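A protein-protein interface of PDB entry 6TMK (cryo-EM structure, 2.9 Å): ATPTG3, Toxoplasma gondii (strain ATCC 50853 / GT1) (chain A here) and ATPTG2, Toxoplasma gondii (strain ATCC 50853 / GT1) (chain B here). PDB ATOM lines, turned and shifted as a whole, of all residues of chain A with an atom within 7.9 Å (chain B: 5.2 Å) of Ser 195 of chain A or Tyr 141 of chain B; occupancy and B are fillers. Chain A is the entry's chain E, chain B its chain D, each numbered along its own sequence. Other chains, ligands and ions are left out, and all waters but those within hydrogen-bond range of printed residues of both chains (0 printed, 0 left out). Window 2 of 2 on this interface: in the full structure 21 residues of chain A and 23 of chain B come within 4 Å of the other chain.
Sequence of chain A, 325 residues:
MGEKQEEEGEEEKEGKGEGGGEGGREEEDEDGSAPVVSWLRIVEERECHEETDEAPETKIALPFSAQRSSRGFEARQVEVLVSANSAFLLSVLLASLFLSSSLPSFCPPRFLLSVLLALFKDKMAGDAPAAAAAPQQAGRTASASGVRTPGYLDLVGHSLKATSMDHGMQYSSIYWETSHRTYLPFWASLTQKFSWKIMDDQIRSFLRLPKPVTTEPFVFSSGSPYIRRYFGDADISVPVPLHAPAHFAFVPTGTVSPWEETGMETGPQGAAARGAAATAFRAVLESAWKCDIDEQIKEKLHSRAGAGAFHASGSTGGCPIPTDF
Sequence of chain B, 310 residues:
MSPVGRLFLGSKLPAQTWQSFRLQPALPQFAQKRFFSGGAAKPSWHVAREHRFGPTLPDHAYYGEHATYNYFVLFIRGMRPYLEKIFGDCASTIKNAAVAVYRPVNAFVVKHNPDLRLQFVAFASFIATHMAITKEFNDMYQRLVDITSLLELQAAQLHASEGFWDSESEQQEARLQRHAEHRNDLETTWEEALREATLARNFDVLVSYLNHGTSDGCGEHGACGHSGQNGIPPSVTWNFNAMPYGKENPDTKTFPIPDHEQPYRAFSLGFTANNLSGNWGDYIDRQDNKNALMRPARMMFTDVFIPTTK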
ATOM      1  N   GLN A 192     -20.489  21.560   2.912  1.00  0.00           N
ATOM      2  CA  GLN A 192     -21.323  20.964   3.945  1.00  0.00           C
ATOM      3  C   GLN A 192     -21.316  19.450   3.800  1.00  0.00           C
ATOM      4  O   GLN A 192     -21.002  18.905   2.739  1.00  0.00           O
ATOM      5  CB  GLN A 192     -22.756  21.493   3.906  1.00  0.00           C
ATOM      6  CG  GLN A 192     -23.493  21.231   2.634  1.00  0.00           C
ATOM      7  CD  GLN A 192     -24.860  21.870   2.639  1.00  0.00           C
ATOM      8  OE1 GLN A 192     -25.487  22.014   3.686  1.00  0.00           O
ATOM      9  NE2 GLN A 192     -25.328  22.263   1.470  1.00  0.00           N
ATOM     10  N   LYS A 193     -21.668  18.778   4.892  1.00  0.00           N
ATOM     11  CA  LYS A 193     -21.602  17.330   4.980  1.00  0.00           C
ATOM     12  C   LYS A 193     -22.789  16.682   4.273  1.00  0.00           C
ATOM     13  O   LYS A 193     -23.711  17.349   3.795  1.00  0.00           O
ATOM     14  CB  LYS A 193     -21.566  16.902   6.442  1.00  0.00           C
ATOM     15  CG  LYS A 193     -20.430  17.489   7.229  1.00  0.00           C
ATOM     16  CD  LYS A 193     -20.203  16.756   8.531  1.00  0.00           C
ATOM     17  CE  LYS A 193     -21.361  16.937   9.482  1.00  0.00           C
ATOM     18  NZ  LYS A 193     -21.736  18.333   9.763  1.00  0.00           N
ATOM     19  N   PHE A 194     -22.768  15.355   4.221  1.00  0.00           N
ATOM     20  CA  PHE A 194     -23.841  14.589   3.612  1.00  0.00           C
ATOM     21  C   PHE A 194     -23.664  13.125   3.972  1.00  0.00           C
ATOM     22  O   PHE A 194     -22.536  12.628   4.014  1.00  0.00           O
ATOM     23  CB  PHE A 194     -23.827  14.759   2.091  1.00  0.00           C
ATOM     24  CG  PHE A 194     -24.975  14.110   1.395  1.00  0.00           C
ATOM     25  CD1 PHE A 194     -26.232  14.670   1.434  1.00  0.00           C
ATOM     26  CD2 PHE A 194     -24.796  12.935   0.698  1.00  0.00           C
ATOM     27  CE1 PHE A 194     -27.284  14.069   0.796  1.00  0.00           C
ATOM     28  CE2 PHE A 194     -25.840  12.338   0.057  1.00  0.00           C
ATOM     29  CZ  PHE A 194     -27.087  12.901   0.105  1.00  0.00           C
ATOM     30  N   SER A 195     -24.775  12.446   4.235  1.00  0.00           N
ATOM     31  CA  SER A 195     -24.792  11.004   4.415  1.00  0.00           C
ATOM     32  C   SER A 195     -25.786  10.381   3.451  1.00  0.00           C
ATOM     33  O   SER A 195     -26.865  10.930   3.211  1.00  0.00           O
ATOM     34  CB  SER A 195     -25.151  10.611   5.847  1.00  0.00           C
ATOM     35  OG  SER A 195     -24.916   9.233   6.053  1.00  0.00           O
ATOM     36  N   TRP A 196     -25.412   9.234   2.898  1.00  0.00           N
ATOM     37  CA  TRP A 196     -26.272   8.492   1.991  1.00  0.00           C
ATOM     38  C   TRP A 196     -27.313   7.656   2.714  1.00  0.00           C
ATOM     39  O   TRP A 196     -28.047   6.913   2.056  1.00  0.00           O
ATOM     40  CB  TRP A 196     -25.437   7.582   1.098  1.00  0.00           C
ATOM     41  CG  TRP A 196     -24.572   8.276   0.122  1.00  0.00           C
ATOM     42  CD1 TRP A 196     -23.218   8.348   0.135  1.00  0.00           C
ATOM     43  CD2 TRP A 196     -24.999   8.986  -1.040  1.00  0.00           C
ATOM     44  NE1 TRP A 196     -22.771   9.061  -0.941  1.00  0.00           N
ATOM     45  CE2 TRP A 196     -23.848   9.465  -1.681  1.00  0.00           C
ATOM     46  CE3 TRP A 196     -26.244   9.265  -1.599  1.00  0.00           C
ATOM     47  CZ2 TRP A 196     -23.905  10.208  -2.849  1.00  0.00           C
ATOM     48  CZ3 TRP A 196     -26.294  10.000  -2.755  1.00  0.00           C
ATOM     49  CH2 TRP A 196     -25.136  10.463  -3.368  1.00  0.00           C
ATOM     50  N   LYS A 197     -27.399   7.752   4.039  1.00  0.00           N
ATOM     51  CA  LYS A 197     -28.207   6.806   4.798  1.00  0.00           C
ATOM     52  C   LYS A 197     -29.694   7.056   4.589  1.00  0.00           C
ATOM     53  O   LYS A 197     -30.477   6.106   4.480  1.00  0.00           O
ATOM     54  CB  LYS A 197     -27.838   6.883   6.276  1.00  0.00           C
ATOM     55  CG  LYS A 197     -28.745   6.096   7.181  1.00  0.00           C
ATOM     56  CD  LYS A 197     -28.031   5.659   8.431  1.00  0.00           C
ATOM     57  CE  LYS A 197     -29.017   5.234   9.495  1.00  0.00           C
ATOM     58  NZ  LYS A 197     -29.801   4.058   9.063  1.00  0.00           N
ATOM     59  N   ILE A 198     -30.104   8.321   4.510  1.00  0.00           N
ATOM     60  CA  ILE A 198     -31.519   8.627   4.332  1.00  0.00           C
ATOM     61  C   ILE A 198     -31.988   8.159   2.960  1.00  0.00           C
ATOM     62  O   ILE A 198     -33.044   7.525   2.820  1.00  0.00           O
ATOM     63  CB  ILE A 198     -31.761  10.136   4.512  1.00  0.00           C
ATOM     64  CG1 ILE A 198     -31.103  10.663   5.790  1.00  0.00           C
ATOM     65  CG2 ILE A 198     -33.243  10.436   4.525  1.00  0.00           C
ATOM     66  CD1 ILE A 198     -31.486   9.946   7.045  1.00  0.00           C
ATOM     67  N   MET A 199     -31.214   8.485   1.925  1.00  0.00           N
ATOM     68  CA  MET A 199     -31.520   8.029   0.577  1.00  0.00           C
ATOM     69  C   MET A 199     -31.545   6.510   0.495  1.00  0.00           C
ATOM     70  O   MET A 199     -32.425   5.927  -0.150  1.00  0.00           O
ATOM     71  CB  MET A 199     -30.494   8.597  -0.394  1.00  0.00           C
ATOM     72  CG  MET A 199     -30.886   8.475  -1.835  1.00  0.00           C
ATOM     73  SD  MET A 199     -29.624   9.104  -2.949  1.00  0.00           S
ATOM     74  CE  MET A 199     -29.807  10.853  -2.658  1.00  0.00           C
ATOM     75  N   ASP A 200     -30.578   5.851   1.132  1.00  0.00           N
ATOM     76  CA  ASP A 200     -30.541   4.395   1.134  1.00  0.00           C
ATOM     77  C   ASP A 200     -31.780   3.815   1.795  1.00  0.00           C
ATOM     78  O   ASP A 200     -32.329   2.813   1.328  1.00  0.00           O
ATOM     79  CB  ASP A 200     -29.283   3.909   1.846  1.00  0.00           C
ATOM     80  CG  ASP A 200     -28.026   4.135   1.031  1.00  0.00           C
ATOM     81  OD1 ASP A 200     -28.129   4.684  -0.084  1.00  0.00           O
ATOM     82  OD2 ASP A 200     -26.932   3.766   1.509  1.00  0.00           O
ATOM     83  N   ASP A 201     -32.233   4.431   2.883  1.00  0.00           N
ATOM     84  CA  ASP A 201     -33.431   3.952   3.560  1.00  0.00           C
ATOM     85  C   ASP A 201     -34.654   4.103   2.668  1.00  0.00           C
ATOM     86  O   ASP A 201     -35.474   3.183   2.553  1.00  0.00           O
ATOM     87  CB  ASP A 201     -33.623   4.714   4.866  1.00  0.00           C
ATOM     88  CG  ASP A 201     -32.578   4.364   5.908  1.00  0.00           C
ATOM     89  OD1 ASP A 201     -32.208   5.254   6.701  1.00  0.00           O
ATOM     90  OD2 ASP A 201     -32.127   3.201   5.936  1.00  0.00           O
ATOM     91  N   PHE B 137     -31.578  16.826   3.728  1.00  0.00           N
ATOM     92  CA  PHE B 137     -31.052  15.532   4.160  1.00  0.00           C
ATOM     93  C   PHE B 137     -30.206  15.669   5.423  1.00  0.00           C
ATOM     94  O   PHE B 137     -30.300  14.847   6.350  1.00  0.00           O
ATOM     95  CB  PHE B 137     -30.226  14.910   3.042  1.00  0.00           C
ATOM     96  CG  PHE B 137     -31.043  14.368   1.914  1.00  0.00           C
ATOM     97  CD1 PHE B 137     -31.696  13.163   2.038  1.00  0.00           C
ATOM     98  CD2 PHE B 137     -31.146  15.054   0.725  1.00  0.00           C
ATOM     99  CE1 PHE B 137     -32.441  12.660   1.002  1.00  0.00           C
ATOM    100  CE2 PHE B 137     -31.889  14.555  -0.311  1.00  0.00           C
ATOM    101  CZ  PHE B 137     -32.536  13.358  -0.173  1.00  0.00           C
ATOM    102  N   ASN B 138     -29.369  16.703   5.470  1.00  0.00           N
ATOM    103  CA  ASN B 138     -28.506  16.930   6.618  1.00  0.00           C
ATOM    104  C   ASN B 138     -29.316  17.220   7.867  1.00  0.00           C
ATOM    105  O   ASN B 138     -28.929  16.821   8.965  1.00  0.00           O
ATOM    106  CB  ASN B 138     -27.548  18.073   6.315  1.00  0.00           C
ATOM    107  CG  ASN B 138     -26.468  17.672   5.355  1.00  0.00           C
ATOM    108  OD1 ASN B 138     -26.602  16.693   4.623  1.00  0.00           O
ATOM    109  ND2 ASN B 138     -25.386  18.424   5.347  1.00  0.00           N
ATOM    110  N   ASP B 139     -30.439  17.919   7.725  1.00  0.00           N
ATOM    111  CA  ASP B 139     -31.291  18.196   8.873  1.00  0.00           C
ATOM    112  C   ASP B 139     -31.859  16.904   9.436  1.00  0.00           C
ATOM    113  O   ASP B 139     -31.911  16.713  10.657  1.00  0.00           O
ATOM    114  CB  ASP B 139     -32.410  19.148   8.463  1.00  0.00           C
ATOM    115  CG  ASP B 139     -31.918  20.562   8.239  1.00  0.00           C
ATOM    116  OD1 ASP B 139     -30.686  20.766   8.210  1.00  0.00           O
ATOM    117  OD2 ASP B 139     -32.761  21.471   8.092  1.00  0.00           O
ATOM    118  N   MET B 140     -32.281  15.997   8.557  1.00  0.00           N
ATOM    119  CA  MET B 140     -32.785  14.709   9.032  1.00  0.00           C
ATOM    120  C   MET B 140     -31.709  13.938   9.802  1.00  0.00           C
ATOM    121  O   MET B 140     -31.929  13.476  10.940  1.00  0.00           O
ATOM    122  CB  MET B 140     -33.298  13.895   7.852  1.00  0.00           C
ATOM    123  CG  MET B 140     -34.336  12.874   8.226  1.00  0.00           C
ATOM    124  SD  MET B 140     -35.922  13.593   8.652  1.00  0.00           S
ATOM    125  CE  MET B 140     -36.712  12.142   9.322  1.00  0.00           C
ATOM    126  N   TYR B 141     -30.531  13.793   9.195  1.00  0.00           N
ATOM    127  CA  TYR B 141     -29.451  13.083   9.871  1.00  0.00           C
ATOM    128  C   TYR B 141     -29.043  13.782  11.163  1.00  0.00           C
ATOM    129  O   TYR B 141     -28.689  13.120  12.146  1.00  0.00           O
ATOM    130  CB  TYR B 141     -28.262  12.949   8.929  1.00  0.00           C
ATOM    131  CG  TYR B 141     -27.298  11.853   9.294  1.00  0.00           C
ATOM    132  CD1 TYR B 141     -27.600  10.531   9.046  1.00  0.00           C
ATOM    133  CD2 TYR B 141     -26.082  12.142   9.880  1.00  0.00           C
ATOM    134  CE1 TYR B 141     -26.727   9.533   9.372  1.00  0.00           C
ATOM    135  CE2 TYR B 141     -25.203  11.151  10.210  1.00  0.00           C
ATOM    136  CZ  TYR B 141     -25.524   9.847   9.950  1.00  0.00           C
ATOM    137  OH  TYR B 141     -24.639   8.856  10.283  1.00  0.00           O
ATOM    138  N   GLN B 142     -29.103  15.112  11.184  1.00  0.00           N
ATOM    139  CA  GLN B 142     -28.773  15.865  12.382  1.00  0.00           C
ATOM    140  C   GLN B 142     -29.768  15.588  13.491  1.00  0.00           C
ATOM    141  O   GLN B 142     -29.395  15.550  14.663  1.00  0.00           O
ATOM    142  CB  GLN B 142     -28.718  17.355  12.069  1.00  0.00           C
ATOM    143  CG  GLN B 142     -28.104  18.178  13.170  1.00  0.00           C
ATOM    144  CD  GLN B 142     -26.606  18.042  13.241  1.00  0.00           C
ATOM    145  OE1 GLN B 142     -25.899  18.299  12.269  1.00  0.00           O
ATOM    146  NE2 GLN B 142     -26.109  17.624  14.396  1.00  0.00           N
ATOM    147  N   ARG B 143     -31.042  15.424  13.150  1.00  0.00           N
ATOM    148  CA  ARG B 143     -32.020  15.088  14.176  1.00  0.00           C
ATOM    149  C   ARG B 143     -31.714  13.728  14.787  1.00  0.00           C
ATOM    150  O   ARG B 143     -31.758  13.560  16.017  1.00  0.00           O
ATOM    151  CB  ARG B 143     -33.430  15.120  13.594  1.00  0.00           C
ATOM    152  CG  ARG B 143     -33.936  16.521  13.362  1.00  0.00           C
ATOM    153  CD  ARG B 143     -35.311  16.559  12.740  1.00  0.00           C
ATOM    154  NE  ARG B 143     -35.689  17.933  12.413  1.00  0.00           N
ATOM    155  CZ  ARG B 143     -35.691  18.457  11.191  1.00  0.00           C
ATOM    156  NH1 ARG B 143     -35.349  17.733  10.137  1.00  0.00           N
ATOM    157  NH2 ARG B 143     -36.040  19.722  11.019  1.00  0.00           N
ATOM    158  N   LEU B 144     -31.369  12.750  13.951  1.00  0.00           N
ATOM    159  CA  LEU B 144     -30.972  11.451  14.495  1.00  0.00           C
ATOM    160  C   LEU B 144     -29.766  11.582  15.428  1.00  0.00           C
ATOM    161  O   LEU B 144     -29.752  11.032  16.543  1.00  0.00           O
ATOM    162  CB  LEU B 144     -30.664  10.482  13.360  1.00  0.00           C
ATOM    163  CG  LEU B 144     -31.839  10.055  12.492  1.00  0.00           C
ATOM    164  CD1 LEU B 144     -31.339   9.371  11.252  1.00  0.00           C
ATOM    165  CD2 LEU B 144     -32.730   9.125  13.254  1.00  0.00           C
ATOM    166  N   VAL B 145     -28.737  12.305  14.985  1.00  0.00           N
ATOM    167  CA  VAL B 145     -27.529  12.461  15.791  1.00  0.00           C
ATOM    168  C   VAL B 145     -27.827  13.204  17.089  1.00  0.00           C
ATOM    169  O   VAL B 145     -27.249  12.904  18.141  1.00  0.00           O
ATOM    170  CB  VAL B 145     -26.446  13.181  14.969  1.00  0.00           C
ATOM    171  CG1 VAL B 145     -25.260  13.518  15.835  1.00  0.00           C
ATOM    172  CG2 VAL B 145     -26.016  12.327  13.818  1.00  0.00           C
ATOM    173  N   ASP B 146     -28.715  14.195  17.032  1.00  0.00           N
ATOM    174  CA  ASP B 146     -29.113  14.916  18.232  1.00  0.00           C
ATOM    175  C   ASP B 146     -29.767  13.980  19.232  1.00  0.00           C
ATOM    176  O   ASP B 146     -29.523  14.076  20.439  1.00  0.00           O
ATOM    177  CB  ASP B 146     -30.055  16.059  17.868  1.00  0.00           C
ATOM    178  CG  ASP B 146     -29.351  17.184  17.140  1.00  0.00           C
ATOM    179  OD1 ASP B 146     -29.921  17.712  16.163  1.00  0.00           O
ATOM    180  OD2 ASP B 146     -28.225  17.545  17.543  1.00  0.00           O
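Among the printed residues, pairs that only touch across the chains: Gln 192 of chain A with Asn 138 of chain B (3.96 Å), Phe 194 of chain A with Phe 137 of chain B (3.8 Å), Phe 194 of chain A with Asn 138 of chain B (3.6 Å), Ser 195 of chain A with Tyr 141 of chain B (3.8 Å) and Ile 198 of chain A with Phe 137 of chain B (3.9 Å).
Of the 10 printed residues of chain A, 5 touch a printed residue of chain B.
Printed residues of chain A that touch a printed residue of chain B: Gln 192, Lys 193, Phe 194, Ser 195 and Ile 198.
Hydrophobic or aromatic side chains of chain A that line the printed part of chain B: Phe 194 and Ile 198.
Hydrophobic or aromatic side chains of chain B within 4 Å of the printed part of chain A: Phe 137 and Tyr 141.
Among the printed residues, 6 pairs touch across the chains.
Among the printed residues, no Asp or Glu carboxylate lies within 4 Å of a Lys or Arg side-chain nitrogen of the other chain.
ND2 of Asn 138 of chain B is in hydrogen-bond range of O of Lys 193 of chain A (2.5 Å).
Ser 195 of chain A touches just one residue of chain B: Tyr 141 (3.8 Å).
Tyr 141 of chain B touches just one residue of chain A: Ser 195 (3.8 Å).
Of the printed residues of chain A, Phe 137 of chain B touches Phe 194 (3.8 Å) and Ile 198 (3.9 Å).
Printed residues of chain B within 4 Å of Ile 198 of chain A: Phe 137 (3.9 Å).
Gln 142 of chain B touches none of the printed residues of chain A.
The nearest residue of chain B that does not touch Ser 195 of chain A is Asn 138 of chain B (4.6 Å).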
